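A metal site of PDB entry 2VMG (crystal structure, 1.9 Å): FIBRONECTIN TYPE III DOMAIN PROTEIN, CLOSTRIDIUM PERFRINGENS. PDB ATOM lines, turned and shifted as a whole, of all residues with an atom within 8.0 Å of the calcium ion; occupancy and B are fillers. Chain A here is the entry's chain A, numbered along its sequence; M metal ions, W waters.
The side-chain hydroxyl (OG) of Ser 143 lies close to the backbone NH (N) of Gly 145 (3.3 Å). The side-chain carboxylate (OD1) of Asp 139 sits close to the backbone NH (N) of Gly 141 (3.1 Å). N of Ala 63 lies within hydrogen-bond range of O of Asp 147 (3.1 Å). The backbone carbonyl oxygen (O) of Ser 96 sits close to the backbone NH (N) of Gly 140 (3.4 Å).
The nearest printed residue that does not touch the calcium ion is Gly 140 (4.3 Å).
The calcium ion is bound by the backbone carbonyl oxygen (O) of Ser 143, 2.3 Å away. Water W1 is bound to the calcium ion. OD1 of Asp 142 binds the calcium ion. The backbone carbonyl oxygen (O) of Asp 139 is bound to the calcium ion (2.4 Å). OD2 of Asp 147 is bound to the calcium ion, 2.5 Å away. The calcium ion is bound by O of Ser 96 (2.6 Å). The calcium ion is bound by the side-chain carboxylate (OD1) of Asp 147 (2.6 Å). OG of Ser 96 binds the calcium ion (2.7 Å). The calcium ion has eight donor atoms within binding distance.
Water W1 bridges O of Gly 145 (2.7 Å) and O of Val 94 (3.0 Å).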
ATOM      1  N   HIS A  62       1.722  -4.317  -1.774  1.00  0.00           N
ATOM      2  CA  HIS A  62       2.094  -3.226  -0.870  1.00  0.00           C
ATOM      3  C   HIS A  62       1.141  -2.046  -1.061  1.00  0.00           C
ATOM      4  O   HIS A  62       0.863  -1.633  -2.195  1.00  0.00           O
ATOM      5  CB  HIS A  62       3.531  -2.785  -1.189  1.00  0.00           C
ATOM      6  CG  HIS A  62       4.209  -2.037  -0.084  1.00  0.00           C
ATOM      7  ND1 HIS A  62       3.859  -0.745   0.260  1.00  0.00           N
ATOM      8  CD2 HIS A  62       5.225  -2.387   0.741  1.00  0.00           C
ATOM      9  CE1 HIS A  62       4.620  -0.338   1.259  1.00  0.00           C
ATOM     10  NE2 HIS A  62       5.460  -1.315   1.573  1.00  0.00           N
ATOM     11  N   ALA A  63       0.639  -1.488   0.050  1.00  0.00           N
ATOM     12  CA  ALA A  63      -0.172  -0.276   0.015  1.00  0.00           C
ATOM     13  C   ALA A  63       0.632   0.892  -0.601  1.00  0.00           C
ATOM     14  O   ALA A  63       1.823   1.012  -0.338  1.00  0.00           O
ATOM     15  CB  ALA A  63      -0.627   0.091   1.419  1.00  0.00           C
ATOM     16  N   VAL A  94       5.832  -0.909  11.945  1.00  0.00           N
ATOM     17  CA  VAL A  94       4.749   0.086  11.915  1.00  0.00           C
ATOM     18  C   VAL A  94       3.645  -0.250  10.917  1.00  0.00           C
ATOM     19  O   VAL A  94       2.754   0.564  10.680  1.00  0.00           O
ATOM     20  CB  VAL A  94       5.281   1.531  11.626  1.00  0.00           C
ATOM     21  CG1 VAL A  94       6.094   2.059  12.799  1.00  0.00           C
ATOM     22  CG2 VAL A  94       6.077   1.580  10.314  1.00  0.00           C
ATOM     23  N   ALA A  95       3.698  -1.454  10.337  1.00  0.00           N
ATOM     24  CA  ALA A  95       2.721  -1.906   9.336  1.00  0.00           C
ATOM     25  C   ALA A  95       1.268  -1.685   9.757  1.00  0.00           C
ATOM     26  O   ALA A  95       0.838  -2.130  10.824  1.00  0.00           O
ATOM     27  CB  ALA A  95       2.955  -3.378   8.995  1.00  0.00           C
ATOM     28  N   SER A  96       0.525  -0.980   8.905  1.00  0.00           N
ATOM     29  CA  SER A  96      -0.883  -0.701   9.164  1.00  0.00           C
ATOM     30  C   SER A  96      -1.622  -0.527   7.846  1.00  0.00           C
ATOM     31  O   SER A  96      -1.288   0.355   7.047  1.00  0.00           O
ATOM     32  CB  SER A  96      -1.037   0.540  10.055  1.00  0.00           C
ATOM     33  OG  SER A  96      -0.379   1.641   9.481  1.00  0.00           O
ATOM     34  N   ILE A  97      -2.613  -1.387   7.621  1.00  0.00           N
ATOM     35  CA  ILE A  97      -3.306  -1.469   6.326  1.00  0.00           C
ATOM     36  C   ILE A  97      -4.780  -1.864   6.460  1.00  0.00           C
ATOM     37  O   ILE A  97      -5.224  -2.289   7.528  1.00  0.00           O
ATOM     38  CB  ILE A  97      -2.617  -2.503   5.374  1.00  0.00           C
ATOM     39  CG1 ILE A  97      -2.540  -3.891   6.023  1.00  0.00           C
ATOM     40  CG2 ILE A  97      -1.233  -2.003   4.948  1.00  0.00           C
ATOM     41  CD1 ILE A  97      -1.927  -4.973   5.142  1.00  0.00           C
ATOM     42  N   SER A  98      -5.522  -1.717   5.367  1.00  0.00           N
ATOM     43  CA  SER A  98      -6.847  -2.306   5.240  1.00  0.00           C
ATOM     44  C   SER A  98      -6.987  -2.998   3.885  1.00  0.00           C
ATOM     45  O   SER A  98      -6.340  -2.615   2.915  1.00  0.00           O
ATOM     46  CB  SER A  98      -7.948  -1.272   5.436  1.00  0.00           C
ATOM     47  OG  SER A  98      -7.952  -0.315   4.391  1.00  0.00           O
ATOM     48  N   LEU A 113      -8.732  -1.732   9.929  1.00  0.00           N
ATOM     49  CA  LEU A 113      -7.310  -1.565  10.237  1.00  0.00           C
ATOM     50  C   LEU A 113      -6.683  -2.868  10.716  1.00  0.00           C
ATOM     51  O   LEU A 113      -7.169  -3.496  11.659  1.00  0.00           O
ATOM     52  CB  LEU A 113      -7.115  -0.450  11.279  1.00  0.00           C
ATOM     53  CG  LEU A 113      -5.705  -0.097  11.772  1.00  0.00           C
ATOM     54  CD1 LEU A 113      -4.774   0.380  10.643  1.00  0.00           C
ATOM     55  CD2 LEU A 113      -5.775   0.944  12.875  1.00  0.00           C
ATOM     56  N   MET A 114      -5.626  -3.290  10.014  1.00  0.00           N
ATOM     57  CA  MET A 114      -4.825  -4.433  10.413  1.00  0.00           C
ATOM     58  C   MET A 114      -3.392  -3.974  10.625  1.00  0.00           C
ATOM     59  O   MET A 114      -2.822  -3.261   9.786  1.00  0.00           O
ATOM     60  CB  MET A 114      -4.880  -5.541   9.358  1.00  0.00           C
ATOM     61  CG  MET A 114      -6.279  -5.995   8.972  1.00  0.00           C
ATOM     62  SD  MET A 114      -6.281  -7.425   7.872  1.00  0.00           S
ATOM     63  CE  MET A 114      -6.144  -8.750   9.073  1.00  0.00           C
ATOM     64  N   THR A 115      -2.809  -4.378  11.748  1.00  0.00           N
ATOM     65  CA  THR A 115      -1.410  -4.056  12.057  1.00  0.00           C
ATOM     66  C   THR A 115      -0.579  -5.337  12.144  1.00  0.00           C
ATOM     67  O   THR A 115      -1.065  -6.415  11.790  1.00  0.00           O
ATOM     68  CB  THR A 115      -1.273  -3.152  13.312  1.00  0.00           C
ATOM     69  OG1 THR A 115      -2.053  -3.684  14.395  1.00  0.00           O
ATOM     70  CG2 THR A 115      -1.750  -1.748  13.012  1.00  0.00           C
ATOM     71  N   LYS A 138      -5.080  -0.613   1.282  1.00  0.00           N
ATOM     72  CA  LYS A 138      -4.873   0.780   1.666  1.00  0.00           C
ATOM     73  C   LYS A 138      -3.831   0.928   2.787  1.00  0.00           C
ATOM     74  O   LYS A 138      -3.421  -0.070   3.381  1.00  0.00           O
ATOM     75  CB  LYS A 138      -6.197   1.440   2.028  1.00  0.00           C
ATOM     76  CG  LYS A 138      -7.045   1.741   0.806  1.00  0.00           C
ATOM     77  CD  LYS A 138      -8.538   1.755   1.110  1.00  0.00           C
ATOM     78  CE  LYS A 138      -9.025   3.132   1.489  1.00  0.00           C
ATOM     79  NZ  LYS A 138     -10.440   3.316   1.058  1.00  0.00           N
ATOM     80  N   ASP A 139      -3.426   2.159   3.063  1.00  0.00           N
ATOM     81  CA  ASP A 139      -2.237   2.439   3.869  1.00  0.00           C
ATOM     82  C   ASP A 139      -2.493   2.685   5.366  1.00  0.00           C
ATOM     83  O   ASP A 139      -1.600   3.161   6.079  1.00  0.00           O
ATOM     84  CB  ASP A 139      -1.453   3.616   3.273  1.00  0.00           C
ATOM     85  CG  ASP A 139      -2.111   4.965   3.525  1.00  0.00           C
ATOM     86  OD1 ASP A 139      -3.307   4.999   3.859  1.00  0.00           O
ATOM     87  OD2 ASP A 139      -1.415   5.989   3.391  1.00  0.00           O
ATOM     88  N   GLY A 140      -3.684   2.371   5.846  1.00  0.00           N
ATOM     89  CA  GLY A 140      -4.005   2.500   7.264  1.00  0.00           C
ATOM     90  C   GLY A 140      -4.196   3.933   7.758  1.00  0.00           C
ATOM     91  O   GLY A 140      -4.497   4.148   8.932  1.00  0.00           O
ATOM     92  N   GLY A 141      -4.001   4.897   6.869  1.00  0.00           N
ATOM     93  CA  GLY A 141      -4.225   6.311   7.191  1.00  0.00           C
ATOM     94  C   GLY A 141      -3.049   7.085   7.767  1.00  0.00           C
ATOM     95  O   GLY A 141      -3.215   8.231   8.206  1.00  0.00           O
ATOM     96  N   ASP A 142      -1.865   6.477   7.764  1.00  0.00           N
ATOM     97  CA  ASP A 142      -0.637   7.149   8.223  1.00  0.00           C
ATOM     98  C   ASP A 142       0.372   7.341   7.075  1.00  0.00           C
ATOM     99  O   ASP A 142       0.520   8.454   6.562  1.00  0.00           O
ATOM    100  CB  ASP A 142       0.008   6.433   9.417  1.00  0.00           C
ATOM    101  CG  ASP A 142      -0.172   4.920   9.377  1.00  0.00           C
ATOM    102  OD1 ASP A 142       0.042   4.292   8.312  1.00  0.00           O
ATOM    103  OD2 ASP A 142      -0.503   4.345  10.440  1.00  0.00           O
ATOM    104  N   SER A 143       1.065   6.262   6.711  1.00  0.00           N
ATOM    105  CA  SER A 143       1.975   6.242   5.568  1.00  0.00           C
ATOM    106  C   SER A 143       2.073   4.808   5.070  1.00  0.00           C
ATOM    107  O   SER A 143       1.572   3.880   5.732  1.00  0.00           O
ATOM    108  CB  SER A 143       3.372   6.754   5.949  1.00  0.00           C
ATOM    109  OG  SER A 143       4.098   5.792   6.701  1.00  0.00           O
ATOM    110  N   ILE A 144       2.714   4.599   3.922  1.00  0.00           N
ATOM    111  CA  ILE A 144       2.900   3.258   3.361  1.00  0.00           C
ATOM    112  C   ILE A 144       4.066   2.481   3.980  1.00  0.00           C
ATOM    113  O   ILE A 144       4.346   1.353   3.584  1.00  0.00           O
ATOM    114  CB  ILE A 144       3.025   3.269   1.812  1.00  0.00           C
ATOM    115  CG1 ILE A 144       4.355   3.918   1.368  1.00  0.00           C
ATOM    116  CG2 ILE A 144       1.796   3.938   1.164  1.00  0.00           C
ATOM    117  CD1 ILE A 144       4.877   3.367   0.053  1.00  0.00           C
ATOM    118  N   GLY A 145       4.742   3.090   4.960  1.00  0.00           N
ATOM    119  CA  GLY A 145       5.880   2.461   5.612  1.00  0.00           C
ATOM    120  C   GLY A 145       5.524   1.108   6.217  1.00  0.00           C
ATOM    121  O   GLY A 145       4.605   1.022   7.038  1.00  0.00           O
ATOM    122  N   SER A 146       6.235   0.065   5.789  1.00  0.00           N
ATOM    123  CA  SER A 146       6.048  -1.315   6.279  1.00  0.00           C
ATOM    124  C   SER A 146       4.760  -2.000   5.803  1.00  0.00           C
ATOM    125  O   SER A 146       4.461  -3.129   6.213  1.00  0.00           O
ATOM    126  CB  SER A 146       6.136  -1.368   7.821  1.00  0.00           C
ATOM    127  OG  SER A 146       7.404  -0.939   8.277  1.00  0.00           O
ATOM    128  N   ASP A 147       4.015  -1.355   4.910  1.00  0.00           N
ATOM    129  CA  ASP A 147       2.667  -1.793   4.556  1.00  0.00           C
ATOM    130  C   ASP A 147       2.615  -2.976   3.577  1.00  0.00           C
ATOM    131  O   ASP A 147       2.016  -2.864   2.506  1.00  0.00           O
ATOM    132  CB  ASP A 147       1.858  -0.632   4.009  1.00  0.00           C
ATOM    133  CG  ASP A 147       1.408   0.348   5.091  1.00  0.00           C
ATOM    134  OD1 ASP A 147       1.803   0.183   6.267  1.00  0.00           O
ATOM    135  OD2 ASP A 147       0.658   1.280   4.760  1.00  0.00           O
ATOM    136  N   HIS A 148       3.224  -4.094   3.958  1.00  0.00           N
ATOM    137  CA  HIS A 148       3.194  -5.311   3.139  1.00  0.00           C
ATOM    138  C   HIS A 148       1.886  -6.057   3.383  1.00  0.00           C
ATOM    139  O   HIS A 148       1.652  -6.590   4.481  1.00  0.00           O
ATOM    140  CB  HIS A 148       4.390  -6.214   3.463  1.00  0.00           C
ATOM    141  CG  HIS A 148       5.735  -5.571   3.274  1.00  0.00           C
ATOM    142  ND1 HIS A 148       6.863  -6.300   2.961  1.00  0.00           N
ATOM    143  CD2 HIS A 148       6.139  -4.273   3.356  1.00  0.00           C
ATOM    144  CE1 HIS A 148       7.903  -5.479   2.863  1.00  0.00           C
ATOM    145  NE2 HIS A 148       7.483  -4.250   3.088  1.00  0.00           N
HETATM  146 CA    CA M   1       0.456   2.344   6.999  1.00  0.00          CA
HETATM  147  O   HOH W   1       2.438   2.093   8.167  1.00  0.00           O
